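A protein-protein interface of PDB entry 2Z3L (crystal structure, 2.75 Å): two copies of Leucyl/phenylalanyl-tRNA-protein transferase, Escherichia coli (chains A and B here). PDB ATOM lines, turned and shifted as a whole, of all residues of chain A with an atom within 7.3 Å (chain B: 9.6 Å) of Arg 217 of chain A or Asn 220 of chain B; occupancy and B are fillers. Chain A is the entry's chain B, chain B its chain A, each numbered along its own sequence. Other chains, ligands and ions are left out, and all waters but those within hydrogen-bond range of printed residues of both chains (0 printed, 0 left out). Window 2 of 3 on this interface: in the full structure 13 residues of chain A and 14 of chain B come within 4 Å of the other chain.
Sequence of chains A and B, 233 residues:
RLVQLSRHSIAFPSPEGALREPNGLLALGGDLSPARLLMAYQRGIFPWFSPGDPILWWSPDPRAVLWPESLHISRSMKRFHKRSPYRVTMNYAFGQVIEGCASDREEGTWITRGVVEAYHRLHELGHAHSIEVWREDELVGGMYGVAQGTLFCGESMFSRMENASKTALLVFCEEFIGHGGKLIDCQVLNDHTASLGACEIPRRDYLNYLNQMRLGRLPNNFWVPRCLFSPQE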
ATOM      1  N   GLN A 148      -2.199 -24.245   7.209  1.00  0.00           N
ATOM      2  CA  GLN A 148      -0.819 -23.897   7.472  1.00  0.00           C
ATOM      3  C   GLN A 148      -0.815 -23.192   8.830  1.00  0.00           C
ATOM      4  O   GLN A 148      -0.384 -22.044   8.950  1.00  0.00           O
ATOM      5  CB  GLN A 148      -0.358 -22.928   6.382  1.00  0.00           C
ATOM      6  CG  GLN A 148       1.115 -22.958   6.032  1.00  0.00           C
ATOM      7  CD  GLN A 148       1.541 -24.286   5.457  1.00  0.00           C
ATOM      8  OE1 GLN A 148       0.747 -24.971   4.831  1.00  0.00           O
ATOM      9  NE2 GLN A 148       2.804 -24.654   5.660  1.00  0.00           N
ATOM     10  N   GLY A 149      -1.303 -23.875   9.858  1.00  0.00           N
ATOM     11  CA  GLY A 149      -1.364 -23.249  11.166  1.00  0.00           C
ATOM     12  C   GLY A 149      -2.609 -22.375  11.207  1.00  0.00           C
ATOM     13  O   GLY A 149      -3.712 -22.853  10.928  1.00  0.00           O
ATOM     14  N   THR A 150      -2.438 -21.097  11.535  1.00  0.00           N
ATOM     15  CA  THR A 150      -3.560 -20.164  11.598  1.00  0.00           C
ATOM     16  C   THR A 150      -3.831 -19.561  10.217  1.00  0.00           C
ATOM     17  O   THR A 150      -4.634 -18.634  10.068  1.00  0.00           O
ATOM     18  CB  THR A 150      -3.285 -19.020  12.612  1.00  0.00           C
ATOM     19  OG1 THR A 150      -2.131 -18.279  12.199  1.00  0.00           O
ATOM     20  CG2 THR A 150      -3.040 -19.584  14.012  1.00  0.00           C
ATOM     21  N   HIS A 179     -11.875 -19.184  16.380  1.00  0.00           N
ATOM     22  CA  HIS A 179     -10.897 -20.031  17.049  1.00  0.00           C
ATOM     23  C   HIS A 179      -9.445 -19.687  16.787  1.00  0.00           C
ATOM     24  O   HIS A 179      -8.566 -20.509  17.018  1.00  0.00           O
ATOM     25  CB  HIS A 179     -11.147 -21.497  16.691  1.00  0.00           C
ATOM     26  CG  HIS A 179     -12.376 -22.062  17.327  1.00  0.00           C
ATOM     27  ND1 HIS A 179     -13.325 -22.771  16.621  1.00  0.00           N
ATOM     28  CD2 HIS A 179     -12.821 -22.005  18.605  1.00  0.00           C
ATOM     29  CE1 HIS A 179     -14.303 -23.123  17.436  1.00  0.00           C
ATOM     30  NE2 HIS A 179     -14.023 -22.670  18.644  1.00  0.00           N
ATOM     31  N   GLY A 180      -9.183 -18.486  16.294  1.00  0.00           N
ATOM     32  CA  GLY A 180      -7.802 -18.112  16.075  1.00  0.00           C
ATOM     33  C   GLY A 180      -7.309 -18.037  14.650  1.00  0.00           C
ATOM     34  O   GLY A 180      -6.207 -17.527  14.420  1.00  0.00           O
ATOM     35  N   GLY A 181      -8.096 -18.547  13.701  1.00  0.00           N
ATOM     36  CA  GLY A 181      -7.691 -18.497  12.304  1.00  0.00           C
ATOM     37  C   GLY A 181      -7.466 -17.051  11.916  1.00  0.00           C
ATOM     38  O   GLY A 181      -8.331 -16.212  12.171  1.00  0.00           O
ATOM     39  N   MET A 213       2.247 -17.583  10.702  1.00  0.00           N
ATOM     40  CA  MET A 213       1.040 -18.293  11.063  1.00  0.00           C
ATOM     41  C   MET A 213       1.183 -19.813  10.966  1.00  0.00           C
ATOM     42  O   MET A 213       0.333 -20.558  11.475  1.00  0.00           O
ATOM     43  CB  MET A 213      -0.110 -17.785  10.188  1.00  0.00           C
ATOM     44  CG  MET A 213      -0.294 -16.268  10.276  1.00  0.00           C
ATOM     45  SD  MET A 213      -1.518 -15.580   9.129  1.00  0.00           S
ATOM     46  CE  MET A 213      -0.873 -14.017   8.795  1.00  0.00           C
ATOM     47  N   ARG A 214       2.260 -20.283  10.337  1.00  0.00           N
ATOM     48  CA  ARG A 214       2.446 -21.728  10.207  1.00  0.00           C
ATOM     49  C   ARG A 214       2.822 -22.421  11.506  1.00  0.00           C
ATOM     50  O   ARG A 214       2.625 -23.628  11.641  1.00  0.00           O
ATOM     51  CB  ARG A 214       3.468 -22.075   9.121  1.00  0.00           C
ATOM     52  CG  ARG A 214       4.798 -21.378   9.214  1.00  0.00           C
ATOM     53  CD  ARG A 214       5.689 -21.809   8.051  1.00  0.00           C
ATOM     54  NE  ARG A 214       6.387 -23.060   8.329  1.00  0.00           N
ATOM     55  CZ  ARG A 214       7.529 -23.132   9.004  1.00  0.00           C
ATOM     56  NH1 ARG A 214       8.102 -22.025   9.461  1.00  0.00           N
ATOM     57  NH2 ARG A 214       8.095 -24.311   9.230  1.00  0.00           N
ATOM     58  N   LEU A 215       3.350 -21.666  12.464  1.00  0.00           N
ATOM     59  CA  LEU A 215       3.721 -22.248  13.753  1.00  0.00           C
ATOM     60  C   LEU A 215       2.669 -21.963  14.826  1.00  0.00           C
ATOM     61  O   LEU A 215       2.894 -22.205  16.009  1.00  0.00           O
ATOM     62  CB  LEU A 215       5.085 -21.728  14.210  1.00  0.00           C
ATOM     63  CG  LEU A 215       6.274 -21.986  13.285  1.00  0.00           C
ATOM     64  CD1 LEU A 215       7.522 -21.350  13.880  1.00  0.00           C
ATOM     65  CD2 LEU A 215       6.452 -23.489  13.091  1.00  0.00           C
ATOM     66  N   GLY A 216       1.527 -21.435  14.398  1.00  0.00           N
ATOM     67  CA  GLY A 216       0.434 -21.164  15.313  1.00  0.00           C
ATOM     68  C   GLY A 216      -0.522 -22.344  15.259  1.00  0.00           C
ATOM     69  O   GLY A 216      -0.316 -23.280  14.484  1.00  0.00           O
ATOM     70  N   ARG A 217      -1.572 -22.319  16.065  1.00  0.00           N
ATOM     71  CA  ARG A 217      -2.510 -23.431  16.060  1.00  0.00           C
ATOM     72  C   ARG A 217      -3.924 -23.107  16.534  1.00  0.00           C
ATOM     73  O   ARG A 217      -4.141 -22.170  17.303  1.00  0.00           O
ATOM     74  CB  ARG A 217      -1.943 -24.581  16.893  1.00  0.00           C
ATOM     75  CG  ARG A 217      -1.301 -24.117  18.174  1.00  0.00           C
ATOM     76  CD  ARG A 217      -1.097 -25.264  19.124  1.00  0.00           C
ATOM     77  NE  ARG A 217      -2.373 -25.850  19.508  1.00  0.00           N
ATOM     78  CZ  ARG A 217      -2.596 -26.452  20.669  1.00  0.00           C
ATOM     79  NH1 ARG A 217      -1.621 -26.548  21.563  1.00  0.00           N
ATOM     80  NH2 ARG A 217      -3.797 -26.947  20.939  1.00  0.00           N
ATOM     81  N   LEU A 218      -4.871 -23.908  16.045  1.00  0.00           N
ATOM     82  CA  LEU A 218      -6.286 -23.794  16.369  1.00  0.00           C
ATOM     83  C   LEU A 218      -6.578 -24.878  17.414  1.00  0.00           C
ATOM     84  O   LEU A 218      -5.703 -25.672  17.745  1.00  0.00           O
ATOM     85  CB  LEU A 218      -7.111 -24.025  15.095  1.00  0.00           C
ATOM     86  CG  LEU A 218      -6.633 -23.204  13.886  1.00  0.00           C
ATOM     87  CD1 LEU A 218      -7.327 -23.631  12.609  1.00  0.00           C
ATOM     88  CD2 LEU A 218      -6.903 -21.750  14.151  1.00  0.00           C
ATOM     89  N   PRO A 219      -7.801 -24.921  17.961  1.00  0.00           N
ATOM     90  CA  PRO A 219      -8.073 -25.961  18.959  1.00  0.00           C
ATOM     91  C   PRO A 219      -7.732 -27.359  18.427  1.00  0.00           C
ATOM     92  O   PRO A 219      -7.980 -27.666  17.256  1.00  0.00           O
ATOM     93  CB  PRO A 219      -9.566 -25.795  19.231  1.00  0.00           C
ATOM     94  CG  PRO A 219      -9.777 -24.333  19.014  1.00  0.00           C
ATOM     95  CD  PRO A 219      -8.978 -24.061  17.765  1.00  0.00           C
ATOM     96  N   ASN A 220      -7.174 -28.197  19.298  1.00  0.00           N
ATOM     97  CA  ASN A 220      -6.777 -29.561  18.947  1.00  0.00           C
ATOM     98  C   ASN A 220      -7.803 -30.407  18.202  1.00  0.00           C
ATOM     99  O   ASN A 220      -7.451 -31.366  17.507  1.00  0.00           O
ATOM    100  CB  ASN A 220      -6.329 -30.295  20.208  1.00  0.00           C
ATOM    101  CG  ASN A 220      -4.856 -30.101  20.485  1.00  0.00           C
ATOM    102  OD1 ASN A 220      -4.220 -29.215  19.899  1.00  0.00           O
ATOM    103  ND2 ASN A 220      -4.300 -30.917  21.375  1.00  0.00           N
ATOM    104  N   ASN A 221      -9.068 -30.044  18.345  1.00  0.00           N
ATOM    105  CA  ASN A 221     -10.152 -30.764  17.702  1.00  0.00           C
ATOM    106  C   ASN A 221     -10.766 -29.922  16.593  1.00  0.00           C
ATOM    107  O   ASN A 221     -11.838 -30.246  16.079  1.00  0.00           O
ATOM    108  CB  ASN A 221     -11.215 -31.109  18.741  1.00  0.00           C
ATOM    109  CG  ASN A 221     -11.607 -29.905  19.592  1.00  0.00           C
ATOM    110  OD1 ASN A 221     -12.489 -29.998  20.448  1.00  0.00           O
ATOM    111  ND2 ASN A 221     -10.947 -28.762  19.359  1.00  0.00           N
ATOM    112  N   PHE A 222     -10.085 -28.840  16.224  1.00  0.00           N
ATOM    113  CA  PHE A 222     -10.598 -27.969  15.181  1.00  0.00           C
ATOM    114  C   PHE A 222     -10.897 -28.658  13.835  1.00  0.00           C
ATOM    115  O   PHE A 222     -11.967 -28.442  13.258  1.00  0.00           O
ATOM    116  CB  PHE A 222      -9.652 -26.787  14.947  1.00  0.00           C
ATOM    117  CG  PHE A 222     -10.220 -25.754  14.022  1.00  0.00           C
ATOM    118  CD1 PHE A 222     -11.256 -24.921  14.441  1.00  0.00           C
ATOM    119  CD2 PHE A 222      -9.795 -25.675  12.696  1.00  0.00           C
ATOM    120  CE1 PHE A 222     -11.865 -24.026  13.552  1.00  0.00           C
ATOM    121  CE2 PHE A 222     -10.399 -24.783  11.791  1.00  0.00           C
ATOM    122  CZ  PHE A 222     -11.437 -23.958  12.223  1.00  0.00           C
ATOM    123  N   MET B  90       8.105 -33.092  11.785  1.00  0.00           N
ATOM    124  CA  MET B  90       7.213 -33.502  12.853  1.00  0.00           C
ATOM    125  C   MET B  90       5.795 -33.454  12.342  1.00  0.00           C
ATOM    126  O   MET B  90       5.404 -32.505  11.687  1.00  0.00           O
ATOM    127  CB  MET B  90       7.343 -32.574  14.049  1.00  0.00           C
ATOM    128  CG  MET B  90       6.533 -33.022  15.245  1.00  0.00           C
ATOM    129  SD  MET B  90       6.531 -31.747  16.508  1.00  0.00           S
ATOM    130  CE  MET B  90       7.984 -32.204  17.488  1.00  0.00           C
ATOM    131  N   LEU B 125      -6.862 -36.204  17.320  1.00  0.00           N
ATOM    132  CA  LEU B 125      -7.260 -35.450  18.502  1.00  0.00           C
ATOM    133  C   LEU B 125      -6.089 -34.708  19.127  1.00  0.00           C
ATOM    134  O   LEU B 125      -6.272 -33.959  20.082  1.00  0.00           O
ATOM    135  CB  LEU B 125      -7.907 -36.372  19.546  1.00  0.00           C
ATOM    136  CG  LEU B 125      -9.198 -37.097  19.132  1.00  0.00           C
ATOM    137  CD1 LEU B 125      -9.685 -37.999  20.259  1.00  0.00           C
ATOM    138  CD2 LEU B 125     -10.265 -36.075  18.772  1.00  0.00           C
ATOM    139  N   GLY B 126      -4.888 -34.935  18.597  1.00  0.00           N
ATOM    140  CA  GLY B 126      -3.702 -34.248  19.092  1.00  0.00           C
ATOM    141  C   GLY B 126      -2.892 -34.844  20.233  1.00  0.00           C
ATOM    142  O   GLY B 126      -2.148 -34.124  20.896  1.00  0.00           O
ATOM    143  N   HIS B 127      -3.008 -36.147  20.460  1.00  0.00           N
ATOM    144  CA  HIS B 127      -2.265 -36.797  21.538  1.00  0.00           C
ATOM    145  C   HIS B 127      -1.135 -37.696  21.066  1.00  0.00           C
ATOM    146  O   HIS B 127      -0.176 -37.941  21.798  1.00  0.00           O
ATOM    147  CB  HIS B 127      -3.214 -37.594  22.418  1.00  0.00           C
ATOM    148  CG  HIS B 127      -4.240 -36.746  23.089  1.00  0.00           C
ATOM    149  ND1 HIS B 127      -5.525 -36.614  22.608  1.00  0.00           N
ATOM    150  CD2 HIS B 127      -4.149 -35.923  24.160  1.00  0.00           C
ATOM    151  CE1 HIS B 127      -6.180 -35.743  23.353  1.00  0.00           C
ATOM    152  NE2 HIS B 127      -5.366 -35.308  24.301  1.00  0.00           N
ATOM    153  N   HIS B 129       1.780 -38.286  18.204  1.00  0.00           N
ATOM    154  CA  HIS B 129       2.535 -37.491  17.256  1.00  0.00           C
ATOM    155  C   HIS B 129       3.590 -38.341  16.574  1.00  0.00           C
ATOM    156  O   HIS B 129       3.958 -39.414  17.062  1.00  0.00           O
ATOM    157  CB  HIS B 129       3.184 -36.330  18.002  1.00  0.00           C
ATOM    158  CG  HIS B 129       2.260 -35.670  18.976  1.00  0.00           C
ATOM    159  ND1 HIS B 129       1.221 -34.854  18.581  1.00  0.00           N
ATOM    160  CD2 HIS B 129       2.181 -35.753  20.325  1.00  0.00           C
ATOM    161  CE1 HIS B 129       0.542 -34.464  19.646  1.00  0.00           C
ATOM    162  NE2 HIS B 129       1.102 -34.996  20.718  1.00  0.00           N
ATOM    163  N   HIS B 179      12.953 -27.847  24.688  1.00  0.00           N
ATOM    164  CA  HIS B 179      11.750 -27.166  25.148  1.00  0.00           C
ATOM    165  C   HIS B 179      11.105 -27.691  26.427  1.00  0.00           C
ATOM    166  O   HIS B 179       9.924 -27.448  26.669  1.00  0.00           O
ATOM    167  CB  HIS B 179      10.698 -27.148  24.036  1.00  0.00           C
ATOM    168  CG  HIS B 179      11.098 -26.356  22.828  1.00  0.00           C
ATOM    169  ND1 HIS B 179      12.165 -26.704  22.027  1.00  0.00           N
ATOM    170  CD2 HIS B 179      10.543 -25.262  22.255  1.00  0.00           C
ATOM    171  CE1 HIS B 179      12.247 -25.863  21.012  1.00  0.00           C
ATOM    172  NE2 HIS B 179      11.272 -24.978  21.127  1.00  0.00           N
ATOM    173  N   ARG B 217       4.150 -29.010  31.022  1.00  0.00           N
ATOM    174  CA  ARG B 217       3.669 -28.499  29.751  1.00  0.00           C
ATOM    175  C   ARG B 217       4.809 -27.999  28.880  1.00  0.00           C
ATOM    176  O   ARG B 217       5.727 -27.340  29.359  1.00  0.00           O
ATOM    177  CB  ARG B 217       2.661 -27.367  30.001  1.00  0.00           C
ATOM    178  CG  ARG B 217       2.019 -26.838  28.732  1.00  0.00           C
ATOM    179  CD  ARG B 217       1.272 -25.531  28.944  1.00  0.00           C
ATOM    180  NE  ARG B 217       1.266 -24.755  27.703  1.00  0.00           N
ATOM    181  CZ  ARG B 217       0.571 -23.638  27.502  1.00  0.00           C
ATOM    182  NH1 ARG B 217      -0.198 -23.140  28.465  1.00  0.00           N
ATOM    183  NH2 ARG B 217       0.649 -23.017  26.334  1.00  0.00           N
ATOM    184  N   LEU B 218       4.747 -28.328  27.596  1.00  0.00           N
ATOM    185  CA  LEU B 218       5.763 -27.901  26.639  1.00  0.00           C
ATOM    186  C   LEU B 218       5.258 -26.627  25.958  1.00  0.00           C
ATOM    187  O   LEU B 218       4.161 -26.148  26.258  1.00  0.00           O
ATOM    188  CB  LEU B 218       5.980 -28.986  25.580  1.00  0.00           C
ATOM    189  CG  LEU B 218       6.423 -30.381  26.015  1.00  0.00           C
ATOM    190  CD1 LEU B 218       6.529 -31.272  24.796  1.00  0.00           C
ATOM    191  CD2 LEU B 218       7.758 -30.300  26.734  1.00  0.00           C
ATOM    192  N   PRO B 219       6.058 -26.042  25.048  1.00  0.00           N
ATOM    193  CA  PRO B 219       5.562 -24.833  24.395  1.00  0.00           C
ATOM    194  C   PRO B 219       4.211 -25.182  23.805  1.00  0.00           C
ATOM    195  O   PRO B 219       4.009 -26.299  23.332  1.00  0.00           O
ATOM    196  CB  PRO B 219       6.612 -24.570  23.324  1.00  0.00           C
ATOM    197  CG  PRO B 219       7.869 -25.009  23.995  1.00  0.00           C
ATOM    198  CD  PRO B 219       7.454 -26.314  24.657  1.00  0.00           C
ATOM    199  N   ASN B 220       3.279 -24.243  23.847  1.00  0.00           N
ATOM    200  CA  ASN B 220       1.950 -24.497  23.320  1.00  0.00           C
ATOM    201  C   ASN B 220       1.947 -25.018  21.887  1.00  0.00           C
ATOM    202  O   ASN B 220       1.121 -25.859  21.537  1.00  0.00           O
ATOM    203  CB  ASN B 220       1.093 -23.234  23.398  1.00  0.00           C
ATOM    204  CG  ASN B 220      -0.293 -23.431  22.792  1.00  0.00           C
ATOM    205  OD1 ASN B 220      -0.462 -23.404  21.568  1.00  0.00           O
ATOM    206  ND2 ASN B 220      -1.293 -23.647  23.650  1.00  0.00           N
ATOM    207  N   ASN B 221       2.873 -24.531  21.066  1.00  0.00           N
ATOM    208  CA  ASN B 221       2.942 -24.941  19.662  1.00  0.00           C
ATOM    209  C   ASN B 221       3.994 -26.002  19.363  1.00  0.00           C
ATOM    210  O   ASN B 221       4.250 -26.308  18.203  1.00  0.00           O
ATOM    211  CB  ASN B 221       3.204 -23.716  18.787  1.00  0.00           C
ATOM    212  CG  ASN B 221       4.572 -23.110  19.032  1.00  0.00           C
ATOM    213  OD1 ASN B 221       5.180 -23.332  20.084  1.00  0.00           O
ATOM    214  ND2 ASN B 221       5.061 -22.328  18.068  1.00  0.00           N
ATOM    215  N   PHE B 222       4.595 -26.566  20.405  1.00  0.00           N
ATOM    216  CA  PHE B 222       5.630 -27.584  20.241  1.00  0.00           C
ATOM    217  C   PHE B 222       5.312 -28.710  19.254  1.00  0.00           C
ATOM    218  O   PHE B 222       6.215 -29.187  18.571  1.00  0.00           O
ATOM    219  CB  PHE B 222       5.981 -28.216  21.589  1.00  0.00           C
ATOM    220  CG  PHE B 222       7.080 -29.232  21.505  1.00  0.00           C
ATOM    221  CD1 PHE B 222       8.413 -28.829  21.410  1.00  0.00           C
ATOM    222  CD2 PHE B 222       6.784 -30.587  21.439  1.00  0.00           C
ATOM    223  CE1 PHE B 222       9.438 -29.760  21.242  1.00  0.00           C
ATOM    224  CE2 PHE B 222       7.798 -31.526  21.274  1.00  0.00           C
ATOM    225  CZ  PHE B 222       9.133 -31.106  21.172  1.00  0.00           C
ATOM    226  N   TRP B 223       4.048 -29.136  19.177  1.00  0.00           N
ATOM    227  CA  TRP B 223       3.672 -30.234  18.275  1.00  0.00           C
ATOM    228  C   TRP B 223       3.085 -29.872  16.914  1.00  0.00           C
ATOM    229  O   TRP B 223       2.655 -30.763  16.181  1.00  0.00           O
ATOM    230  CB  TRP B 223       2.695 -31.199  18.957  1.00  0.00           C
ATOM    231  CG  TRP B 223       3.199 -31.837  20.208  1.00  0.00           C
ATOM    232  CD1 TRP B 223       2.793 -31.571  21.482  1.00  0.00           C
ATOM    233  CD2 TRP B 223       4.176 -32.883  20.308  1.00  0.00           C
ATOM    234  NE1 TRP B 223       3.448 -32.387  22.373  1.00  0.00           N
ATOM    235  CE2 TRP B 223       4.304 -33.203  21.681  1.00  0.00           C
ATOM    236  CE3 TRP B 223       4.956 -33.578  19.375  1.00  0.00           C
ATOM    237  CZ2 TRP B 223       5.180 -34.191  22.142  1.00  0.00           C
ATOM    238  CZ3 TRP B 223       5.828 -34.560  19.834  1.00  0.00           C
ATOM    239  CH2 TRP B 223       5.931 -34.857  21.206  1.00  0.00           C
ATOM    240  N   VAL B 224       3.049 -28.592  16.564  1.00  0.00           N
ATOM    241  CA  VAL B 224       2.505 -28.220  15.260  1.00  0.00           C
ATOM    242  C   VAL B 224       3.408 -28.857  14.217  1.00  0.00           C
ATOM    243  O   VAL B 224       4.609 -29.010  14.427  1.00  0.00           O
ATOM    244  CB  VAL B 224       2.504 -26.689  15.022  1.00  0.00           C
ATOM    245  CG1 VAL B 224       1.833 -25.971  16.180  1.00  0.00           C
ATOM    246  CG2 VAL B 224       3.929 -26.190  14.825  1.00  0.00           C
ATOM    247  N   PRO B 225       2.842 -29.262  13.083  1.00  0.00           N
ATOM    248  CA  PRO B 225       3.712 -29.872  12.080  1.00  0.00           C
ATOM    249  C   PRO B 225       4.721 -28.886  11.499  1.00  0.00           C
ATOM    250  O   PRO B 225       4.381 -27.751  11.163  1.00  0.00           O
ATOM    251  CB  PRO B 225       2.721 -30.406  11.047  1.00  0.00           C
ATOM    252  CG  PRO B 225       1.527 -29.517  11.224  1.00  0.00           C
ATOM    253  CD  PRO B 225       1.428 -29.372  12.703  1.00  0.00           C
ATOM    254  N   ARG B 226       5.971 -29.329  11.401  1.00  0.00           N
ATOM    255  CA  ARG B 226       7.057 -28.513  10.863  1.00  0.00           C
ATOM    256  C   ARG B 226       8.282 -29.351  10.536  1.00  0.00           C
ATOM    257  O   ARG B 226       8.295 -30.571  10.702  1.00  0.00           O
ATOM    258  CB  ARG B 226       7.473 -27.456  11.874  1.00  0.00           C
ATOM    259  CG  ARG B 226       7.935 -28.031  13.203  1.00  0.00           C
ATOM    260  CD  ARG B 226       7.208 -27.330  14.321  1.00  0.00           C
ATOM    261  NE  ARG B 226       7.447 -27.892  15.644  1.00  0.00           N
ATOM    262  CZ  ARG B 226       8.565 -27.716  16.330  1.00  0.00           C
ATOM    263  NH1 ARG B 226       9.550 -26.997  15.798  1.00  0.00           N
ATOM    264  NH2 ARG B 226       8.680 -28.228  17.553  1.00  0.00           N
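O of Asn 220 of chain B lies within hydrogen-bond range of NH1 of Arg 217 of chain A, at 2.8 Å.
The backbone carbonyl oxygen (O) of Leu 215 of chain A is in hydrogen-bond range of the side-chain amide nitrogen (ND2) of Asn 221 of chain B (3.0 Å).
The backbone carbonyl oxygen (O) of Gly 126 of chain B sits close to a ring nitrogen (NE2) of His 129 of chain B (3.4 Å).
The side-chain amide nitrogen (ND2) of Asn 220 of chain B lies close to the guanidinium group (NH2) of Arg 217 of chain B (3.4 Å).
NE of Arg 226 of chain B lies close to O of Val 224 of chain B, 3.3 Å away.
NH2 of Arg 217 of chain A is in hydrogen-bond range of OD1 of Asn 220 of chain A.
Leu 215 of chain A touches Val 224 of chain B.
Gly 216 of chain A touches Val 224 of chain B (O to CG1, 3.8 Å).
Leu 125 of chain B touches Asn 220 of chain A.
ND2 of Asn 220 of chain A touches O of Gly 126 of chain B, at 3.9 Å.
Arg 217 of chain A touches just one residue of chain B: Asn 220.
Asn 220 of chain B touches one residue of chain A.
Printed residues of chain B within 4 Å of Gly 216 of chain A: Val 224.
Of the printed residues of chain A, Val 224 of chain B touches Leu 215 (3.9 Å) and Gly 216 (3.8 Å).
Printed residues of chain B within 4 Å of Asn 220 of chain A: Leu 125 and Gly 126.
Of the printed residues of chain A, Gly 126 of chain B touches Asn 220.
Of the printed residues of chain A, Leu 125 of chain B touches Asn 220.
Of the printed residues of chain B, Leu 215 of chain A touches Asn 221 (3.0 Å) and Val 224 (3.9 Å).
Pro 219 of chain A touches none of the printed residues of chain B.
The nearest residue of chain A that does not touch Asn 220 of chain B is Gly 216 of chain A (6.4 Å).
Hydrophobic or aromatic side chains of chain A that line the printed part of chain B: Leu 215.
Along chain A the printed residues that touch a printed residue of chain B span positions 215 to 220.
Printed residues of chain B that touch a printed residue of chain A: Leu 125, Gly 126, Asn 220, Asn 221 and Val 224.
Hydrophobic or aromatic side chains of chain B that line the printed part of chain A: Val 224.
Among the printed residues, 6 pairs touch across the chains.
Among the printed residues, no Asp or Glu carboxylate lies within 4 Å of a Lys or Arg side-chain nitrogen of the other chain.
Arg 217 of chain A touches Asn 220 of chain B, but with the chains exchanged Asn 220 of chain A does not touch Arg 217 of chain B (10.2 Å).
Positions printed for both chains: 179, 217, 218, 219, 220, 221 and 222.
Of the 6 pairs that touch across the chains among the printed residues, none has its exchanged pair printed and touching as well.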
